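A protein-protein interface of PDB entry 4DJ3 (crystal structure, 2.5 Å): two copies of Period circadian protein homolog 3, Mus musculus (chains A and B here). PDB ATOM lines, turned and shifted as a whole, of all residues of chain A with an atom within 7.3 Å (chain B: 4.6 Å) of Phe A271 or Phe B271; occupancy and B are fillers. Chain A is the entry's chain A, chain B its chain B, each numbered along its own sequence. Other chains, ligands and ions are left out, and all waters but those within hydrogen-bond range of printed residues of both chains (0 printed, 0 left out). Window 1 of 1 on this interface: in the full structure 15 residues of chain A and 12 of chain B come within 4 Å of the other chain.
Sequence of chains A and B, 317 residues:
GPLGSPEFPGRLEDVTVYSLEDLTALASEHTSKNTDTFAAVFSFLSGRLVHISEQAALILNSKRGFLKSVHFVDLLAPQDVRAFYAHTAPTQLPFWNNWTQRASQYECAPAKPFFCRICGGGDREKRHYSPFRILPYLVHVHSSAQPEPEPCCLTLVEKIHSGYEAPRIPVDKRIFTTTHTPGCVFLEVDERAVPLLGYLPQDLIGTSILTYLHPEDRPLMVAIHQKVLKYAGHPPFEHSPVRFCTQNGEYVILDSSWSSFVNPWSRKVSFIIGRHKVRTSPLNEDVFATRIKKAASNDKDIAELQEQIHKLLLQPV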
ATOM      1  N   THR A 178      25.261 -10.830 -27.450  1.00  0.00           N
ATOM      2  CA  THR A 178      26.201 -11.833 -27.971  1.00  0.00           C
ATOM      3  C   THR A 178      26.376 -12.854 -26.898  1.00  0.00           C
ATOM      4  O   THR A 178      26.138 -12.555 -25.719  1.00  0.00           O
ATOM      5  CB  THR A 178      27.592 -11.270 -28.183  1.00  0.00           C
ATOM      6  OG1 THR A 178      28.112 -10.835 -26.920  1.00  0.00           O
ATOM      7  CG2 THR A 178      27.575 -10.095 -29.148  1.00  0.00           C
ATOM      8  N   THR A 179      26.793 -14.051 -27.288  1.00  0.00           N
ATOM      9  CA  THR A 179      27.197 -15.029 -26.309  1.00  0.00           C
ATOM     10  C   THR A 179      28.550 -15.580 -26.663  1.00  0.00           C
ATOM     11  O   THR A 179      28.917 -15.606 -27.838  1.00  0.00           O
ATOM     12  CB  THR A 179      26.193 -16.213 -26.097  1.00  0.00           C
ATOM     13  OG1 THR A 179      25.931 -16.894 -27.328  1.00  0.00           O
ATOM     14  CG2 THR A 179      24.946 -15.765 -25.484  1.00  0.00           C
ATOM     15  N   HIS A 180      29.305 -15.986 -25.643  1.00  0.00           N
ATOM     16  CA  HIS A 180      30.617 -16.559 -25.858  1.00  0.00           C
ATOM     17  C   HIS A 180      30.997 -17.697 -24.905  1.00  0.00           C
ATOM     18  O   HIS A 180      30.522 -17.767 -23.786  1.00  0.00           O
ATOM     19  CB  HIS A 180      31.679 -15.480 -25.984  1.00  0.00           C
ATOM     20  CG  HIS A 180      31.929 -14.675 -24.743  1.00  0.00           C
ATOM     21  ND1 HIS A 180      31.491 -13.375 -24.610  1.00  0.00           N
ATOM     22  CD2 HIS A 180      32.678 -14.936 -23.636  1.00  0.00           C
ATOM     23  CE1 HIS A 180      31.910 -12.885 -23.452  1.00  0.00           C
ATOM     24  NE2 HIS A 180      32.632 -13.809 -22.842  1.00  0.00           N
ATOM     25  N   THR A 181      31.828 -18.600 -25.377  1.00  0.00           N
ATOM     26  CA  THR A 181      32.224 -19.807 -24.628  1.00  0.00           C
ATOM     27  C   THR A 181      33.179 -19.438 -23.480  1.00  0.00           C
ATOM     28  O   THR A 181      33.765 -18.342 -23.464  1.00  0.00           O
ATOM     29  CB  THR A 181      33.027 -20.779 -25.515  1.00  0.00           C
ATOM     30  OG1 THR A 181      34.291 -20.166 -25.791  1.00  0.00           O
ATOM     31  CG2 THR A 181      32.340 -21.038 -26.869  1.00  0.00           C
ATOM     32  N   PRO A 182      33.372 -20.372 -22.525  1.00  0.00           N
ATOM     33  CA  PRO A 182      34.405 -20.100 -21.549  1.00  0.00           C
ATOM     34  C   PRO A 182      35.795 -19.861 -22.152  1.00  0.00           C
ATOM     35  O   PRO A 182      36.687 -19.375 -21.449  1.00  0.00           O
ATOM     36  CB  PRO A 182      34.385 -21.365 -20.673  1.00  0.00           C
ATOM     37  CG  PRO A 182      32.953 -21.840 -20.803  1.00  0.00           C
ATOM     38  CD  PRO A 182      32.714 -21.663 -22.250  1.00  0.00           C
ATOM     39  N   VAL A 185      35.339 -17.472 -27.048  1.00  0.00           N
ATOM     40  CA  VAL A 185      35.021 -17.584 -28.495  1.00  0.00           C
ATOM     41  C   VAL A 185      33.496 -17.272 -28.755  1.00  0.00           C
ATOM     42  O   VAL A 185      32.657 -17.899 -28.115  1.00  0.00           O
ATOM     43  CB  VAL A 185      35.316 -19.016 -28.963  1.00  0.00           C
ATOM     44  CG1 VAL A 185      34.796 -19.248 -30.361  1.00  0.00           C
ATOM     45  CG2 VAL A 185      36.851 -19.370 -28.775  1.00  0.00           C
ATOM     46  N   LEU A 187      29.757 -17.468 -29.664  1.00  0.00           N
ATOM     47  CA  LEU A 187      28.857 -18.488 -30.154  1.00  0.00           C
ATOM     48  C   LEU A 187      27.705 -17.884 -30.957  1.00  0.00           C
ATOM     49  O   LEU A 187      27.157 -18.516 -31.898  1.00  0.00           O
ATOM     50  CB  LEU A 187      28.221 -19.257 -29.013  1.00  0.00           C
ATOM     51  CG  LEU A 187      29.064 -20.213 -28.171  1.00  0.00           C
ATOM     52  CD1 LEU A 187      28.402 -20.286 -26.847  1.00  0.00           C
ATOM     53  CD2 LEU A 187      29.211 -21.636 -28.806  1.00  0.00           C
ATOM     54  N   GLU A 188      27.271 -16.692 -30.561  1.00  0.00           N
ATOM     55  CA  GLU A 188      26.048 -16.198 -31.130  1.00  0.00           C
ATOM     56  C   GLU A 188      26.065 -14.716 -31.178  1.00  0.00           C
ATOM     57  O   GLU A 188      26.547 -14.094 -30.268  1.00  0.00           O
ATOM     58  CB  GLU A 188      24.917 -16.590 -30.241  1.00  0.00           C
ATOM     59  CG  GLU A 188      23.686 -16.876 -31.000  1.00  0.00           C
ATOM     60  CD  GLU A 188      23.365 -18.328 -30.881  1.00  0.00           C
ATOM     61  OE1 GLU A 188      22.441 -18.643 -30.073  1.00  0.00           O
ATOM     62  OE2 GLU A 188      24.089 -19.138 -31.538  1.00  0.00           O
ATOM     63  N   HIS A 225      35.069 -11.621 -16.221  1.00  0.00           N
ATOM     64  CA  HIS A 225      34.789 -13.021 -15.973  1.00  0.00           C
ATOM     65  C   HIS A 225      34.888 -13.405 -14.486  1.00  0.00           C
ATOM     66  O   HIS A 225      34.239 -14.369 -14.060  1.00  0.00           O
ATOM     67  CB  HIS A 225      35.640 -13.887 -16.885  1.00  0.00           C
ATOM     68  CG  HIS A 225      35.134 -13.916 -18.290  1.00  0.00           C
ATOM     69  ND1 HIS A 225      35.356 -12.891 -19.188  1.00  0.00           N
ATOM     70  CD2 HIS A 225      34.389 -14.838 -18.946  1.00  0.00           C
ATOM     71  CE1 HIS A 225      34.792 -13.197 -20.341  1.00  0.00           C
ATOM     72  NE2 HIS A 225      34.192 -14.367 -20.217  1.00  0.00           N
ATOM     73  N   VAL A 228      31.646 -12.658 -13.516  1.00  0.00           N
ATOM     74  CA  VAL A 228      30.737 -13.646 -14.062  1.00  0.00           C
ATOM     75  C   VAL A 228      30.514 -14.787 -13.070  1.00  0.00           C
ATOM     76  O   VAL A 228      29.361 -15.138 -12.837  1.00  0.00           O
ATOM     77  CB  VAL A 228      31.028 -14.061 -15.534  1.00  0.00           C
ATOM     78  CG1 VAL A 228      30.508 -15.436 -15.831  1.00  0.00           C
ATOM     79  CG2 VAL A 228      30.369 -13.057 -16.450  1.00  0.00           C
ATOM     80  N   SER A 259      25.992 -11.593 -17.980  1.00  0.00           N
ATOM     81  CA  SER A 259      25.426 -12.615 -17.164  1.00  0.00           C
ATOM     82  C   SER A 259      25.865 -13.931 -17.731  1.00  0.00           C
ATOM     83  O   SER A 259      26.749 -13.982 -18.599  1.00  0.00           O
ATOM     84  CB  SER A 259      23.893 -12.513 -17.186  1.00  0.00           C
ATOM     85  OG  SER A 259      23.300 -13.300 -16.168  1.00  0.00           O
ATOM     86  N   SER A 260      25.276 -15.010 -17.255  1.00  0.00           N
ATOM     87  CA  SER A 260      25.781 -16.256 -17.731  1.00  0.00           C
ATOM     88  C   SER A 260      24.689 -17.327 -17.752  1.00  0.00           C
ATOM     89  O   SER A 260      23.563 -17.092 -17.284  1.00  0.00           O
ATOM     90  CB  SER A 260      27.013 -16.682 -16.892  1.00  0.00           C
ATOM     91  OG  SER A 260      26.727 -16.700 -15.497  1.00  0.00           O
ATOM     92  N   PHE A 261      25.016 -18.459 -18.365  1.00  0.00           N
ATOM     93  CA  PHE A 261      24.281 -19.683 -18.175  1.00  0.00           C
ATOM     94  C   PHE A 261      25.236 -20.746 -17.633  1.00  0.00           C
ATOM     95  O   PHE A 261      26.189 -21.164 -18.303  1.00  0.00           O
ATOM     96  CB  PHE A 261      23.708 -20.189 -19.505  1.00  0.00           C
ATOM     97  CG  PHE A 261      22.959 -21.481 -19.386  1.00  0.00           C
ATOM     98  CD1 PHE A 261      21.805 -21.567 -18.605  1.00  0.00           C
ATOM     99  CD2 PHE A 261      23.389 -22.600 -20.035  1.00  0.00           C
ATOM    100  CE1 PHE A 261      21.084 -22.767 -18.510  1.00  0.00           C
ATOM    101  CE2 PHE A 261      22.649 -23.831 -19.950  1.00  0.00           C
ATOM    102  CZ  PHE A 261      21.520 -23.894 -19.165  1.00  0.00           C
ATOM    103  N   VAL A 262      24.953 -21.197 -16.425  1.00  0.00           N
ATOM    104  CA  VAL A 262      25.679 -22.313 -15.842  1.00  0.00           C
ATOM    105  C   VAL A 262      24.918 -23.645 -16.048  1.00  0.00           C
ATOM    106  O   VAL A 262      23.713 -23.733 -15.748  1.00  0.00           O
ATOM    107  CB  VAL A 262      26.062 -22.065 -14.330  1.00  0.00           C
ATOM    108  CG1 VAL A 262      26.075 -20.565 -13.984  1.00  0.00           C
ATOM    109  CG2 VAL A 262      25.168 -22.822 -13.445  1.00  0.00           C
ATOM    110  N   ASN A 263      25.627 -24.651 -16.581  1.00  0.00           N
ATOM    111  CA  ASN A 263      25.057 -25.999 -16.827  1.00  0.00           C
ATOM    112  C   ASN A 263      24.412 -26.501 -15.534  1.00  0.00           C
ATOM    113  O   ASN A 263      25.048 -26.508 -14.498  1.00  0.00           O
ATOM    114  CB  ASN A 263      26.146 -26.960 -17.340  1.00  0.00           C
ATOM    115  CG  ASN A 263      25.621 -28.342 -17.628  1.00  0.00           C
ATOM    116  OD1 ASN A 263      25.461 -28.716 -18.784  1.00  0.00           O
ATOM    117  ND2 ASN A 263      25.344 -29.114 -16.579  1.00  0.00           N
ATOM    118  N   LYS A 268      28.917 -25.636 -13.916  1.00  0.00           N
ATOM    119  CA  LYS A 268      29.952 -24.816 -14.534  1.00  0.00           C
ATOM    120  C   LYS A 268      29.370 -23.882 -15.604  1.00  0.00           C
ATOM    121  O   LYS A 268      28.396 -24.218 -16.297  1.00  0.00           O
ATOM    122  CB  LYS A 268      31.014 -25.711 -15.155  1.00  0.00           C
ATOM    123  CG  LYS A 268      31.683 -26.663 -14.148  1.00  0.00           C
ATOM    124  CD  LYS A 268      32.474 -27.762 -14.819  1.00  0.00           C
ATOM    125  CE  LYS A 268      33.212 -27.269 -16.051  1.00  0.00           C
ATOM    126  NZ  LYS A 268      34.439 -28.114 -16.292  1.00  0.00           N
ATOM    127  N   VAL A 269      29.959 -22.697 -15.726  1.00  0.00           N
ATOM    128  CA  VAL A 269      29.574 -21.734 -16.772  1.00  0.00           C
ATOM    129  C   VAL A 269      29.637 -22.297 -18.199  1.00  0.00           C
ATOM    130  O   VAL A 269      30.653 -22.768 -18.670  1.00  0.00           O
ATOM    131  CB  VAL A 269      30.411 -20.501 -16.660  1.00  0.00           C
ATOM    132  CG1 VAL A 269      30.231 -19.627 -17.917  1.00  0.00           C
ATOM    133  CG2 VAL A 269      30.006 -19.735 -15.362  1.00  0.00           C
ATOM    134  N   SER A 270      28.521 -22.266 -18.900  1.00  0.00           N
ATOM    135  CA  SER A 270      28.480 -22.875 -20.203  1.00  0.00           C
ATOM    136  C   SER A 270      28.688 -21.785 -21.248  1.00  0.00           C
ATOM    137  O   SER A 270      29.397 -21.968 -22.237  1.00  0.00           O
ATOM    138  CB  SER A 270      27.170 -23.594 -20.389  1.00  0.00           C
ATOM    139  OG  SER A 270      26.959 -23.759 -21.777  1.00  0.00           O
ATOM    140  N   PHE A 271      28.075 -20.635 -21.035  1.00  0.00           N
ATOM    141  CA  PHE A 271      28.376 -19.537 -21.888  1.00  0.00           C
ATOM    142  C   PHE A 271      28.126 -18.250 -21.157  1.00  0.00           C
ATOM    143  O   PHE A 271      27.430 -18.213 -20.117  1.00  0.00           O
ATOM    144  CB  PHE A 271      27.632 -19.627 -23.231  1.00  0.00           C
ATOM    145  CG  PHE A 271      26.148 -19.488 -23.138  1.00  0.00           C
ATOM    146  CD1 PHE A 271      25.571 -18.282 -22.816  1.00  0.00           C
ATOM    147  CD2 PHE A 271      25.328 -20.589 -23.388  1.00  0.00           C
ATOM    148  CE1 PHE A 271      24.202 -18.176 -22.737  1.00  0.00           C
ATOM    149  CE2 PHE A 271      23.972 -20.510 -23.314  1.00  0.00           C
ATOM    150  CZ  PHE A 271      23.388 -19.294 -23.007  1.00  0.00           C
ATOM    151  N   ILE A 272      28.744 -17.208 -21.679  1.00  0.00           N
ATOM    152  CA  ILE A 272      28.617 -15.875 -21.121  1.00  0.00           C
ATOM    153  C   ILE A 272      27.804 -15.035 -22.096  1.00  0.00           C
ATOM    154  O   ILE A 272      28.046 -15.075 -23.327  1.00  0.00           O
ATOM    155  CB  ILE A 272      30.004 -15.239 -21.000  1.00  0.00           C
ATOM    156  CG1 ILE A 272      31.036 -16.310 -20.568  1.00  0.00           C
ATOM    157  CG2 ILE A 272      29.986 -13.972 -20.142  1.00  0.00           C
ATOM    158  CD1 ILE A 272      31.103 -16.437 -19.141  1.00  0.00           C
ATOM    159  N   ILE A 273      26.896 -14.235 -21.538  1.00  0.00           N
ATOM    160  CA  ILE A 273      26.023 -13.399 -22.332  1.00  0.00           C
ATOM    161  C   ILE A 273      26.073 -11.898 -22.046  1.00  0.00           C
ATOM    162  O   ILE A 273      26.029 -11.459 -20.870  1.00  0.00           O
ATOM    163  CB  ILE A 273      24.570 -13.943 -22.358  1.00  0.00           C
ATOM    164  CG1 ILE A 273      23.774 -13.276 -23.477  1.00  0.00           C
ATOM    165  CG2 ILE A 273      23.882 -13.886 -20.966  1.00  0.00           C
ATOM    166  CD1 ILE A 273      22.397 -14.001 -23.805  1.00  0.00           C
ATOM    167  N   GLY A 274      26.139 -11.126 -23.131  1.00  0.00           N
ATOM    168  CA  GLY A 274      26.216  -9.674 -23.087  1.00  0.00           C
ATOM    169  C   GLY A 274      25.094  -8.964 -23.879  1.00  0.00           C
ATOM    170  O   GLY A 274      24.765  -9.337 -24.986  1.00  0.00           O
ATOM    171  N   THR B 179      18.451 -29.254 -26.257  1.00  0.00           N
ATOM    172  CA  THR B 179      17.882 -27.944 -25.955  1.00  0.00           C
ATOM    173  C   THR B 179      16.858 -27.579 -27.025  1.00  0.00           C
ATOM    174  O   THR B 179      17.018 -27.907 -28.194  1.00  0.00           O
ATOM    175  CB  THR B 179      18.957 -26.780 -25.728  1.00  0.00           C
ATOM    176  OG1 THR B 179      19.623 -26.468 -26.941  1.00  0.00           O
ATOM    177  CG2 THR B 179      20.028 -27.148 -24.710  1.00  0.00           C
ATOM    178  N   HIS B 180      15.792 -26.913 -26.619  1.00  0.00           N
ATOM    179  CA  HIS B 180      14.813 -26.496 -27.595  1.00  0.00           C
ATOM    180  C   HIS B 180      14.253 -25.123 -27.288  1.00  0.00           C
ATOM    181  O   HIS B 180      14.306 -24.670 -26.139  1.00  0.00           O
ATOM    182  CB  HIS B 180      13.700 -27.541 -27.826  1.00  0.00           C
ATOM    183  CG  HIS B 180      12.898 -27.872 -26.612  1.00  0.00           C
ATOM    184  ND1 HIS B 180      13.153 -28.986 -25.834  1.00  0.00           N
ATOM    185  CD2 HIS B 180      11.834 -27.250 -26.047  1.00  0.00           C
ATOM    186  CE1 HIS B 180      12.295 -29.012 -24.822  1.00  0.00           C
ATOM    187  NE2 HIS B 180      11.479 -27.980 -24.934  1.00  0.00           N
ATOM    188  N   LEU B 187      17.487 -27.175 -30.870  1.00  0.00           N
ATOM    189  CA  LEU B 187      18.607 -26.274 -31.105  1.00  0.00           C
ATOM    190  C   LEU B 187      19.881 -27.082 -31.008  1.00  0.00           C
ATOM    191  O   LEU B 187      20.760 -27.016 -31.875  1.00  0.00           O
ATOM    192  CB  LEU B 187      18.669 -25.225 -30.011  1.00  0.00           C
ATOM    193  CG  LEU B 187      17.534 -24.232 -29.973  1.00  0.00           C
ATOM    194  CD1 LEU B 187      17.540 -23.466 -28.655  1.00  0.00           C
ATOM    195  CD2 LEU B 187      17.637 -23.293 -31.217  1.00  0.00           C
ATOM    196  N   SER B 260      15.928 -24.708 -17.646  1.00  0.00           N
ATOM    197  CA  SER B 260      15.772 -23.717 -18.662  1.00  0.00           C
ATOM    198  C   SER B 260      16.799 -22.586 -18.488  1.00  0.00           C
ATOM    199  O   SER B 260      17.394 -22.450 -17.438  1.00  0.00           O
ATOM    200  CB  SER B 260      14.344 -23.177 -18.597  1.00  0.00           C
ATOM    201  OG  SER B 260      14.094 -22.489 -17.375  1.00  0.00           O
ATOM    202  N   PHE B 261      17.004 -21.809 -19.554  1.00  0.00           N
ATOM    203  CA  PHE B 261      17.747 -20.563 -19.502  1.00  0.00           C
ATOM    204  C   PHE B 261      16.788 -19.399 -19.763  1.00  0.00           C
ATOM    205  O   PHE B 261      16.103 -19.354 -20.773  1.00  0.00           O
ATOM    206  CB  PHE B 261      18.928 -20.589 -20.480  1.00  0.00           C
ATOM    207  CG  PHE B 261      19.644 -19.281 -20.600  1.00  0.00           C
ATOM    208  CD1 PHE B 261      20.398 -18.781 -19.545  1.00  0.00           C
ATOM    209  CD2 PHE B 261      19.578 -18.548 -21.772  1.00  0.00           C
ATOM    210  CE1 PHE B 261      21.077 -17.583 -19.651  1.00  0.00           C
ATOM    211  CE2 PHE B 261      20.254 -17.326 -21.886  1.00  0.00           C
ATOM    212  CZ  PHE B 261      20.997 -16.843 -20.812  1.00  0.00           C
ATOM    213  N   VAL B 269      11.638 -17.127 -20.887  1.00  0.00           N
ATOM    214  CA  VAL B 269      12.414 -18.346 -21.128  1.00  0.00           C
ATOM    215  C   VAL B 269      13.083 -18.343 -22.501  1.00  0.00           C
ATOM    216  O   VAL B 269      12.450 -18.096 -23.510  1.00  0.00           O
ATOM    217  CB  VAL B 269      11.544 -19.611 -20.896  1.00  0.00           C
ATOM    218  CG1 VAL B 269      12.129 -20.808 -21.589  1.00  0.00           C
ATOM    219  CG2 VAL B 269      11.366 -19.865 -19.372  1.00  0.00           C
ATOM    220  N   SER B 270      14.375 -18.593 -22.545  1.00  0.00           N
ATOM    221  CA  SER B 270      15.073 -18.519 -23.817  1.00  0.00           C
ATOM    222  C   SER B 270      15.242 -19.869 -24.457  1.00  0.00           C
ATOM    223  O   SER B 270      15.140 -19.983 -25.664  1.00  0.00           O
ATOM    224  CB  SER B 270      16.415 -17.819 -23.668  1.00  0.00           C
ATOM    225  OG  SER B 270      16.984 -17.607 -24.946  1.00  0.00           O
ATOM    226  N   PHE B 271      15.539 -20.884 -23.662  1.00  0.00           N
ATOM    227  CA  PHE B 271      15.530 -22.245 -24.176  1.00  0.00           C
ATOM    228  C   PHE B 271      15.331 -23.200 -23.051  1.00  0.00           C
ATOM    229  O   PHE B 271      15.371 -22.761 -21.888  1.00  0.00           O
ATOM    230  CB  PHE B 271      16.757 -22.597 -25.064  1.00  0.00           C
ATOM    231  CG  PHE B 271      18.090 -22.597 -24.348  1.00  0.00           C
ATOM    232  CD1 PHE B 271      18.474 -23.669 -23.551  1.00  0.00           C
ATOM    233  CD2 PHE B 271      18.989 -21.517 -24.502  1.00  0.00           C
ATOM    234  CE1 PHE B 271      19.724 -23.674 -22.895  1.00  0.00           C
ATOM    235  CE2 PHE B 271      20.248 -21.516 -23.850  1.00  0.00           C
ATOM    236  CZ  PHE B 271      20.607 -22.598 -23.044  1.00  0.00           C
ATOM    237  N   ILE B 272      15.042 -24.467 -23.389  1.00  0.00           N
ATOM    238  CA  ILE B 272      14.747 -25.525 -22.405  1.00  0.00           C
ATOM    239  C   ILE B 272      15.746 -26.608 -22.692  1.00  0.00           C
ATOM    240  O   ILE B 272      15.923 -26.973 -23.855  1.00  0.00           O
ATOM    241  CB  ILE B 272      13.344 -26.203 -22.603  1.00  0.00           C
ATOM    242  CG1 ILE B 272      12.220 -25.249 -23.137  1.00  0.00           C
ATOM    243  CG2 ILE B 272      12.950 -27.122 -21.415  1.00  0.00           C
ATOM    244  CD1 ILE B 272      11.938 -24.080 -22.328  1.00  0.00           C
ATOM    245  N   ILE B 273      16.364 -27.130 -21.624  1.00  0.00           N
ATOM    246  CA  ILE B 273      17.414 -28.148 -21.678  1.00  0.00           C
ATOM    247  C   ILE B 273      16.914 -29.408 -20.983  1.00  0.00           C
ATOM    248  O   ILE B 273      16.382 -29.340 -19.866  1.00  0.00           O
ATOM    249  CB  ILE B 273      18.590 -27.750 -20.778  1.00  0.00           C
ATOM    250  CG1 ILE B 273      18.431 -26.339 -20.279  1.00  0.00           C
ATOM    251  CG2 ILE B 273      20.003 -28.090 -21.372  1.00  0.00           C
ATOM    252  CD1 ILE B 273      18.663 -26.290 -18.811  1.00  0.00           C
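Thr A178 touches none of the printed residues of chain B. Printed residues of chain B within 4 Å of Ser A260: Phe B261. Of the printed residues of chain B, Phe A261 touches Ser B260 (3.9 Å), Phe B261 (3.3 Å), Phe B271 (3.9 Å) and Ile B273 (3.7 Å). Of chain A, only Phe A261 and Phe A271 come within 4 Å of Phe B271. The nearest printed residue of chain B that does not touch Phe A271 is Ser B270 (6.9 Å). The nearest residue of chain A that does not touch Phe B271 is Ser A270 (6.6 Å).
Phe B261 touches its own counterpart, Phe A261. Phe A261 touches Phe B271, and with the chains exchanged Phe A271 touches Phe B261. Phe A261 touches Ile B273, but with the chains exchanged Ile A273 does not touch Phe B261 (4.1 Å). Phe A271 touches its own counterpart, Phe B271. Positions printed for both chains: 179, 180, 187, 260, 261, 269, 270, 271, 272 and 273.
O of Ser A260 touches CE1 of Phe B261, at 3.5 Å. Phe A261 touches Ser B260 (CE1 to O, 3.9 Å). Phe A261 touches Phe B261 (CD1 to CD1, 3.3 Å). Phe A261 touches Phe B271. Phe A261 touches Ile B273. Phe B261 touches Phe A271. Phe A271 touches Phe B271.
Hydrophobic or aromatic side chains of chain A within 4 Å of the printed part of chain B: Phe A261 and Phe A271. Of the 10 printed residues of chain B, 4 touch a printed residue of chain A. Among the printed residues, no Asp or Glu carboxylate lies within 4 Å of a Lys or Arg side-chain nitrogen of the other chain.
O of Phe B261 lies within hydrogen-bond range of N of Ser B270 (2.6 Å). The backbone NH (N) of Phe B261 is in hydrogen-bond range of the backbone carbonyl oxygen (O) of Phe B271 (3.0 Å). N of Ser A270 lies within hydrogen-bond range of O of Phe A261 (2.6 Å). O of Phe A271 sits at hydrogen-bond distance from N of Phe A261 (3.0 Å).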
